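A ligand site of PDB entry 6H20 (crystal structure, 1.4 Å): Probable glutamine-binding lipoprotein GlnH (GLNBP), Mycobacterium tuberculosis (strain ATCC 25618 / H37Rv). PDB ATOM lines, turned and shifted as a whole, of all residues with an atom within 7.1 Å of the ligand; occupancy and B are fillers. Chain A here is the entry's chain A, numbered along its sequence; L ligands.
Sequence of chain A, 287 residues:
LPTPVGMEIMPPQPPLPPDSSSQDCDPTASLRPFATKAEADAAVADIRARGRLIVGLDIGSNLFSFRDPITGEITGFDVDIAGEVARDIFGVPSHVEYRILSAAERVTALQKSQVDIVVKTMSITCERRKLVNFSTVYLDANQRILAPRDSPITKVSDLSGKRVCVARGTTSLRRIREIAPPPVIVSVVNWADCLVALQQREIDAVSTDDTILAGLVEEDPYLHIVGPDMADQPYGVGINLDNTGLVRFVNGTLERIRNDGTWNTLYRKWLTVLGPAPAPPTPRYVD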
ATOM      1  N   SER A  61      28.440   1.931 -10.496  1.00  0.00           N
ATOM      2  CA  SER A  61      27.927   0.977  -9.525  1.00  0.00           C
ATOM      3  C   SER A  61      27.951   1.605  -8.130  1.00  0.00           C
ATOM      4  O   SER A  61      28.935   1.481  -7.391  1.00  0.00           O
ATOM      5  CB  SER A  61      28.730  -0.341  -9.573  1.00  0.00           C
ATOM      6  OG  SER A  61      28.541  -1.008 -10.829  1.00  0.00           O
ATOM      7  N   ALA A 103      31.704  -2.984 -18.004  1.00  0.00           N
ATOM      8  CA  ALA A 103      31.621  -4.417 -17.734  1.00  0.00           C
ATOM      9  C   ALA A 103      32.114  -5.229 -18.917  1.00  0.00           C
ATOM     10  O   ALA A 103      32.796  -6.249 -18.757  1.00  0.00           O
ATOM     11  CB  ALA A 103      30.179  -4.792 -17.395  1.00  0.00           C
ATOM     12  N   ARG A 106      36.196  -5.561 -19.080  1.00  0.00           N
ATOM     13  CA  ARG A 106      37.028  -6.062 -17.996  1.00  0.00           C
ATOM     14  C   ARG A 106      38.017  -7.129 -18.476  1.00  0.00           C
ATOM     15  O   ARG A 106      39.187  -7.102 -18.094  1.00  0.00           O
ATOM     16  CB  ARG A 106      36.161  -6.632 -16.880  1.00  0.00           C
ATOM     17  CG  ARG A 106      35.339  -5.584 -16.161  1.00  0.00           C
ATOM     18  CD  ARG A 106      34.360  -6.227 -15.147  1.00  0.00           C
ATOM     19  NE  ARG A 106      33.298  -6.950 -15.847  1.00  0.00           N
ATOM     20  CZ  ARG A 106      32.211  -7.443 -15.240  1.00  0.00           C
ATOM     21  NH1 ARG A 106      32.079  -7.309 -13.927  1.00  0.00           N
ATOM     22  NH2 ARG A 106      31.280  -8.069 -15.947  1.00  0.00           N
ATOM     23  N   LYS A 120      35.759  -4.962  -9.967  1.00  0.00           N
ATOM     24  CA  LYS A 120      34.529  -4.388 -10.508  1.00  0.00           C
ATOM     25  C   LYS A 120      33.479  -5.477 -10.577  1.00  0.00           C
ATOM     26  O   LYS A 120      33.184  -5.997 -11.661  1.00  0.00           O
ATOM     27  CB  LYS A 120      34.775  -3.763 -11.892  1.00  0.00           C
ATOM     28  CG  LYS A 120      33.602  -2.886 -12.342  1.00  0.00           C
ATOM     29  CD  LYS A 120      33.561  -2.749 -13.848  1.00  0.00           C
ATOM     30  CE  LYS A 120      32.391  -1.885 -14.333  1.00  0.00           C
ATOM     31  NZ  LYS A 120      31.103  -2.105 -13.593  1.00  0.00           N
ATOM     32  N   THR A 121      32.950  -5.833  -9.405  1.00  0.00           N
ATOM     33  CA  THR A 121      31.909  -6.836  -9.230  1.00  0.00           C
ATOM     34  C   THR A 121      32.060  -8.034 -10.178  1.00  0.00           C
ATOM     35  O   THR A 121      31.099  -8.478 -10.808  1.00  0.00           O
ATOM     36  CB  THR A 121      30.498  -6.213  -9.332  1.00  0.00           C
ATOM     37  OG1 THR A 121      30.284  -5.628 -10.643  1.00  0.00           O
ATOM     38  CG2 THR A 121      30.303  -5.125  -8.272  1.00  0.00           C
ATOM     39  N   MET A 122      33.271  -8.562 -10.304  1.00  0.00           N
ATOM     40  CA  MET A 122      33.564  -9.445 -11.431  1.00  0.00           C
ATOM     41  C   MET A 122      33.316 -10.883 -11.038  1.00  0.00           C
ATOM     42  O   MET A 122      34.136 -11.511 -10.352  1.00  0.00           O
ATOM     43  CB  MET A 122      34.986  -9.239 -11.946  1.00  0.00           C
ATOM     44  CG  MET A 122      35.187  -9.845 -13.325  1.00  0.00           C
ATOM     45  SD  MET A 122      36.784  -9.397 -13.973  1.00  0.00           S
ATOM     46  CE  MET A 122      36.710 -10.201 -15.565  1.00  0.00           C
ATOM     47  N   SER A 123      32.186 -11.439 -11.490  1.00  0.00           N
ATOM     48  CA  SER A 123      31.863 -12.827 -11.168  1.00  0.00           C
ATOM     49  C   SER A 123      32.875 -13.780 -11.795  1.00  0.00           C
ATOM     50  O   SER A 123      33.248 -13.660 -12.968  1.00  0.00           O
ATOM     51  CB  SER A 123      30.476 -13.193 -11.673  1.00  0.00           C
ATOM     52  OG  SER A 123      29.513 -12.429 -10.982  1.00  0.00           O
ATOM     53  N   ILE A 124      33.303 -14.747 -10.989  1.00  0.00           N
ATOM     54  CA  ILE A 124      34.256 -15.760 -11.421  1.00  0.00           C
ATOM     55  C   ILE A 124      33.473 -16.850 -12.131  1.00  0.00           C
ATOM     56  O   ILE A 124      32.601 -17.488 -11.529  1.00  0.00           O
ATOM     57  CB  ILE A 124      34.991 -16.341 -10.205  1.00  0.00           C
ATOM     58  CG1 ILE A 124      35.771 -15.271  -9.430  1.00  0.00           C
ATOM     59  CG2 ILE A 124      35.928 -17.481 -10.631  1.00  0.00           C
ATOM     60  CD1 ILE A 124      36.063 -15.676  -7.959  1.00  0.00           C
ATOM     61  N   THR A 125      33.780 -17.081 -13.408  1.00  0.00           N
ATOM     62  CA  THR A 125      33.111 -18.116 -14.179  1.00  0.00           C
ATOM     63  C   THR A 125      34.138 -18.964 -14.924  1.00  0.00           C
ATOM     64  O   THR A 125      35.272 -18.537 -15.161  1.00  0.00           O
ATOM     65  CB  THR A 125      32.121 -17.543 -15.213  1.00  0.00           C
ATOM     66  OG1 THR A 125      32.843 -16.865 -16.247  1.00  0.00           O
ATOM     67  CG2 THR A 125      31.119 -16.577 -14.545  1.00  0.00           C
ATOM     68  N   ARG A 128      35.139 -17.236 -18.188  1.00  0.00           N
ATOM     69  CA  ARG A 128      36.106 -16.158 -17.983  1.00  0.00           C
ATOM     70  C   ARG A 128      37.472 -16.698 -17.601  1.00  0.00           C
ATOM     71  O   ARG A 128      38.495 -16.101 -17.949  1.00  0.00           O
ATOM     72  CB  ARG A 128      35.587 -15.161 -16.949  1.00  0.00           C
ATOM     73  CG  ARG A 128      34.445 -14.310 -17.469  1.00  0.00           C
ATOM     74  CD  ARG A 128      33.795 -13.529 -16.353  1.00  0.00           C
ATOM     75  NE  ARG A 128      32.697 -12.720 -16.893  1.00  0.00           N
ATOM     76  CZ  ARG A 128      31.923 -11.931 -16.150  1.00  0.00           C
ATOM     77  NH1 ARG A 128      32.134 -11.834 -14.841  1.00  0.00           N
ATOM     78  NH2 ARG A 128      30.951 -11.222 -16.723  1.00  0.00           N
ATOM     79  N   ALA A 141      27.442 -12.679  -4.203  1.00  0.00           N
ATOM     80  CA  ALA A 141      26.147 -12.070  -4.470  1.00  0.00           C
ATOM     81  C   ALA A 141      25.258 -13.051  -5.225  1.00  0.00           C
ATOM     82  O   ALA A 141      25.669 -14.168  -5.580  1.00  0.00           O
ATOM     83  CB  ALA A 141      26.327 -10.752  -5.231  1.00  0.00           C
ATOM     84  N   ALA A 167      23.195  -4.683 -18.263  1.00  0.00           N
ATOM     85  CA  ALA A 167      24.385  -4.099 -18.883  1.00  0.00           C
ATOM     86  C   ALA A 167      25.040  -5.109 -19.798  1.00  0.00           C
ATOM     87  O   ALA A 167      25.061  -6.310 -19.520  1.00  0.00           O
ATOM     88  CB  ALA A 167      25.382  -3.648 -17.808  1.00  0.00           C
ATOM     89  N   ARG A 168      25.576  -4.623 -20.912  1.00  0.00           N
ATOM     90  CA  ARG A 168      26.260  -5.506 -21.841  1.00  0.00           C
ATOM     91  C   ARG A 168      27.521  -6.069 -21.194  1.00  0.00           C
ATOM     92  O   ARG A 168      28.148  -5.418 -20.348  1.00  0.00           O
ATOM     93  CB  ARG A 168      26.574  -4.751 -23.146  1.00  0.00           C
ATOM     94  CG  ARG A 168      25.328  -4.550 -24.011  1.00  0.00           C
ATOM     95  CD  ARG A 168      25.647  -3.959 -25.381  1.00  0.00           C
ATOM     96  NE  ARG A 168      26.066  -2.566 -25.308  1.00  0.00           N
ATOM     97  CZ  ARG A 168      25.247  -1.525 -25.162  1.00  0.00           C
ATOM     98  NH1 ARG A 168      23.929  -1.714 -25.039  1.00  0.00           N
ATOM     99  NH2 ARG A 168      25.738  -0.290 -25.126  1.00  0.00           N
ATOM    100  N   GLY A 169      27.862  -7.301 -21.549  1.00  0.00           N
ATOM    101  CA  GLY A 169      29.103  -7.876 -21.057  1.00  0.00           C
ATOM    102  C   GLY A 169      28.992  -8.503 -19.697  1.00  0.00           C
ATOM    103  O   GLY A 169      30.022  -8.735 -19.039  1.00  0.00           O
ATOM    104  N   THR A 170      27.785  -8.805 -19.231  1.00  0.00           N
ATOM    105  CA  THR A 170      27.605  -9.287 -17.869  1.00  0.00           C
ATOM    106  C   THR A 170      27.040 -10.693 -17.854  1.00  0.00           C
ATOM    107  O   THR A 170      26.384 -11.147 -18.799  1.00  0.00           O
ATOM    108  CB  THR A 170      26.660  -8.374 -17.085  1.00  0.00           C
ATOM    109  OG1 THR A 170      25.360  -8.364 -17.700  1.00  0.00           O
ATOM    110  CG2 THR A 170      27.219  -6.957 -16.987  1.00  0.00           C
ATOM    111  N   THR A 171      27.266 -11.385 -16.737  1.00  0.00           N
ATOM    112  CA  THR A 171      26.624 -12.672 -16.528  1.00  0.00           C
ATOM    113  C   THR A 171      25.121 -12.484 -16.404  1.00  0.00           C
ATOM    114  O   THR A 171      24.370 -13.418 -16.711  1.00  0.00           O
ATOM    115  CB  THR A 171      27.116 -13.282 -15.207  1.00  0.00           C
ATOM    116  OG1 THR A 171      26.863 -12.361 -14.139  1.00  0.00           O
ATOM    117  CG2 THR A 171      28.623 -13.652 -15.274  1.00  0.00           C
ATOM    118  N   SER A 172      24.682 -11.286 -16.017  1.00  0.00           N
ATOM    119  CA  SER A 172      23.267 -11.008 -15.821  1.00  0.00           C
ATOM    120  C   SER A 172      22.508 -11.165 -17.132  1.00  0.00           C
ATOM    121  O   SER A 172      21.410 -11.738 -17.158  1.00  0.00           O
ATOM    122  CB  SER A 172      23.098  -9.586 -15.300  1.00  0.00           C
ATOM    123  OG  SER A 172      24.019  -9.326 -14.258  1.00  0.00           O
ATOM    124  N   LEU A 173      23.094 -10.662 -18.219  1.00  0.00           N
ATOM    125  CA  LEU A 173      22.490 -10.809 -19.547  1.00  0.00           C
ATOM    126  C   LEU A 173      22.339 -12.280 -19.897  1.00  0.00           C
ATOM    127  O   LEU A 173      21.287 -12.711 -20.377  1.00  0.00           O
ATOM    128  CB  LEU A 173      23.376 -10.091 -20.570  1.00  0.00           C
ATOM    129  CG  LEU A 173      23.072 -10.253 -22.059  1.00  0.00           C
ATOM    130  CD1 LEU A 173      21.615  -9.974 -22.371  1.00  0.00           C
ATOM    131  CD2 LEU A 173      23.991  -9.346 -22.872  1.00  0.00           C
ATOM    132  N   TRP A 191      25.138  -0.140 -15.077  1.00  0.00           N
ATOM    133  CA  TRP A 191      23.921  -0.347 -14.303  1.00  0.00           C
ATOM    134  C   TRP A 191      23.234   0.968 -13.939  1.00  0.00           C
ATOM    135  O   TRP A 191      22.003   0.988 -13.791  1.00  0.00           O
ATOM    136  CB  TRP A 191      24.222  -1.190 -13.068  1.00  0.00           C
ATOM    137  CG  TRP A 191      24.589  -2.574 -13.481  1.00  0.00           C
ATOM    138  CD1 TRP A 191      25.824  -3.151 -13.413  1.00  0.00           C
ATOM    139  CD2 TRP A 191      23.723  -3.538 -14.089  1.00  0.00           C
ATOM    140  NE1 TRP A 191      25.770  -4.421 -13.916  1.00  0.00           N
ATOM    141  CE2 TRP A 191      24.499  -4.692 -14.342  1.00  0.00           C
ATOM    142  CE3 TRP A 191      22.370  -3.562 -14.433  1.00  0.00           C
ATOM    143  CZ2 TRP A 191      23.987  -5.831 -14.942  1.00  0.00           C
ATOM    144  CZ3 TRP A 191      21.837  -4.694 -15.025  1.00  0.00           C
ATOM    145  CH2 TRP A 191      22.650  -5.831 -15.273  1.00  0.00           C
ATOM    146  N   THR A 208      20.061  -8.057 -11.973  1.00  0.00           N
ATOM    147  CA  THR A 208      21.500  -8.278 -11.804  1.00  0.00           C
ATOM    148  C   THR A 208      21.738  -8.655 -10.355  1.00  0.00           C
ATOM    149  O   THR A 208      20.790  -8.899  -9.584  1.00  0.00           O
ATOM    150  CB  THR A 208      22.341  -7.078 -12.268  1.00  0.00           C
ATOM    151  OG1 THR A 208      23.736  -7.433 -12.248  1.00  0.00           O
ATOM    152  CG2 THR A 208      22.177  -5.848 -11.385  1.00  0.00           C
ATOM    153  N   ASP A 209      23.019  -8.698  -9.965  1.00  0.00           N
ATOM    154  CA  ASP A 209      23.427  -9.045  -8.604  1.00  0.00           C
ATOM    155  C   ASP A 209      22.646  -8.227  -7.586  1.00  0.00           C
ATOM    156  O   ASP A 209      22.509  -7.012  -7.715  1.00  0.00           O
ATOM    157  CB  ASP A 209      24.899  -8.671  -8.427  1.00  0.00           C
ATOM    158  CG  ASP A 209      25.828  -9.232  -9.501  1.00  0.00           C
ATOM    159  OD1 ASP A 209      25.407  -9.992 -10.409  1.00  0.00           O
ATOM    160  OD2 ASP A 209      27.016  -8.877  -9.410  1.00  0.00           O
ATOM    161  N   THR A 211      23.546  -7.240  -4.735  1.00  0.00           N
ATOM    162  CA  THR A 211      24.444  -6.185  -4.259  1.00  0.00           C
ATOM    163  C   THR A 211      24.324  -4.926  -5.105  1.00  0.00           C
ATOM    164  O   THR A 211      24.161  -3.821  -4.570  1.00  0.00           O
ATOM    165  CB  THR A 211      25.876  -6.712  -4.360  1.00  0.00           C
ATOM    166  OG1 THR A 211      26.013  -7.403  -5.606  1.00  0.00           O
ATOM    167  CG2 THR A 211      26.191  -7.692  -3.218  1.00  0.00           C
ATOM    168  N   ILE A 212      24.455  -5.061  -6.432  1.00  0.00           N
ATOM    169  CA  ILE A 212      24.329  -3.915  -7.337  1.00  0.00           C
ATOM    170  C   ILE A 212      22.930  -3.324  -7.240  1.00  0.00           C
ATOM    171  O   ILE A 212      22.756  -2.090  -7.185  1.00  0.00           O
ATOM    172  CB  ILE A 212      24.669  -4.345  -8.782  1.00  0.00           C
ATOM    173  CG1 ILE A 212      26.118  -4.831  -8.871  1.00  0.00           C
ATOM    174  CG2 ILE A 212      24.403  -3.173  -9.771  1.00  0.00           C
ATOM    175  CD1 ILE A 212      26.471  -5.379 -10.248  1.00  0.00           C
ATOM    176  N   GLN A 233      26.814 -15.310  -7.886  1.00  0.00           N
ATOM    177  CA  GLN A 233      27.751 -14.323  -8.441  1.00  0.00           C
ATOM    178  C   GLN A 233      28.912 -14.178  -7.462  1.00  0.00           C
ATOM    179  O   GLN A 233      28.932 -13.273  -6.610  1.00  0.00           O
ATOM    180  CB  GLN A 233      27.058 -12.977  -8.665  1.00  0.00           C
ATOM    181  CG  GLN A 233      25.745 -13.090  -9.444  1.00  0.00           C
ATOM    182  CD  GLN A 233      25.934 -13.490 -10.909  1.00  0.00           C
ATOM    183  OE1 GLN A 233      26.959 -13.223 -11.526  1.00  0.00           O
ATOM    184  NE2 GLN A 233      24.912 -14.121 -11.466  1.00  0.00           N
ATOM    185  N   PRO A 234      29.905 -15.060  -7.547  1.00  0.00           N
ATOM    186  CA  PRO A 234      31.056 -14.964  -6.636  1.00  0.00           C
ATOM    187  C   PRO A 234      32.106 -14.023  -7.191  1.00  0.00           C
ATOM    188  O   PRO A 234      32.724 -14.315  -8.223  1.00  0.00           O
ATOM    189  CB  PRO A 234      31.557 -16.409  -6.575  1.00  0.00           C
ATOM    190  CG  PRO A 234      31.195 -16.993  -7.958  1.00  0.00           C
ATOM    191  CD  PRO A 234      30.019 -16.172  -8.505  1.00  0.00           C
ATOM    192  N   TYR A 235      32.317 -12.875  -6.530  1.00  0.00           N
ATOM    193  CA  TYR A 235      33.230 -11.869  -7.057  1.00  0.00           C
ATOM    194  C   TYR A 235      34.681 -12.243  -6.818  1.00  0.00           C
ATOM    195  O   TYR A 235      35.064 -12.665  -5.730  1.00  0.00           O
ATOM    196  CB  TYR A 235      33.002 -10.525  -6.355  1.00  0.00           C
ATOM    197  CG  TYR A 235      31.683  -9.846  -6.610  1.00  0.00           C
ATOM    198  CD1 TYR A 235      30.742 -10.371  -7.505  1.00  0.00           C
ATOM    199  CD2 TYR A 235      31.372  -8.688  -5.940  1.00  0.00           C
ATOM    200  CE1 TYR A 235      29.510  -9.708  -7.725  1.00  0.00           C
ATOM    201  CE2 TYR A 235      30.172  -8.031  -6.160  1.00  0.00           C
ATOM    202  CZ  TYR A 235      29.252  -8.544  -7.035  1.00  0.00           C
ATOM    203  OH  TYR A 235      28.061  -7.857  -7.229  1.00  0.00           O
HETATM  204  N1  LIG L   1      28.699  -9.607 -11.460  1.00  0.00           N
HETATM  205  C1  LIG L   1      28.113  -9.593 -12.795  1.00  0.00           C
HETATM  206  C2  LIG L   1      29.184  -9.888 -13.828  1.00  0.00           C
HETATM  207  O1  LIG L   1      28.961  -9.708 -15.035  1.00  0.00           O
HETATM  208  C3  LIG L   1      27.432  -8.249 -13.083  1.00  0.00           C
HETATM  209  C4  LIG L   1      28.422  -7.110 -13.200  1.00  0.00           C
HETATM  210  O2  LIG L   1      29.571  -7.214 -12.776  1.00  0.00           O
HETATM  211  N2  LIG L   1      27.982  -6.037 -13.813  1.00  0.00           N
HETATM  212  O3  LIG L   1      30.286 -10.316 -13.424  1.00  0.00           O
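The backbone carbonyl oxygen (O) of Thr 121 is in hydrogen-bond range of a nitrogen (N1) of the ligand (2.7 Å).
O2 of the ligand lies within hydrogen-bond range of OG1 of Thr 121, at 2.8 Å.
NE1 of Trp 191 sits close to N2 of the ligand, 2.7 Å away.
N1 of the ligand is in salt-bridge range of OD2 of Asp 209, 2.8 Å away.
The guanidinium group (NH2) of Arg 106 is in salt-bridge range of an oxygen (O1) of the ligand.
NH1 of Arg 128 is in salt-bridge range of O3 of the ligand (2.8 Å).
The backbone NH (N) of Thr 171 sits at hydrogen-bond distance from an oxygen (O1) of the ligand, 2.9 Å away.
OG1 of Thr 171 sits close to O1 of the ligand (3.5 Å).
The backbone NH of Ser 123 lies within hydrogen-bond range of an oxygen (O3) of the ligand, at 2.9 Å.
The side-chain hydroxyl (OG) of Ser 123 lies within hydrogen-bond range of a nitrogen (N1) of the ligand.
Merely in contact with the ligand: Thr 170, Ser 172, Tyr 235, Thr 208, Met 122, Ile 212 and Lys 120.
Hydrophobic or aromatic side chains within 4 Å of the ligand: Trp 191, Ile 212 and Tyr 235.
The side-chain carboxylate (OD2) of Asp 209 sits at hydrogen-bond distance from the side-chain hydroxyl (OH) of Tyr 235, at 2.6 Å.
The guanidinium group (NH2) of Arg 106 lies within hydrogen-bond range of the backbone carbonyl oxygen (O) of Gly 169, 3.4 Å away.
The guanidinium group (NE) of Arg 106 sits at hydrogen-bond distance from the backbone carbonyl oxygen (O) of Ala 103 (3.0 Å).
The guanidinium group (NH1) of Arg 128 is in hydrogen-bond range of the backbone carbonyl oxygen (O) of Ser 123.
The side-chain hydroxyl of Thr 171 is in hydrogen-bond range of the side-chain amide oxygen of Gln 233 (2.8 Å).
OG of Ser 123 is in hydrogen-bond range of OE1 of Gln 233, 2.7 Å away.
The side-chain hydroxyl of Thr 170 lies within hydrogen-bond range of the backbone carbonyl oxygen of Ala 167, 2.8 Å away.
OG1 of Thr 208 sits at hydrogen-bond distance from OG of Ser 172, at 2.8 Å.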
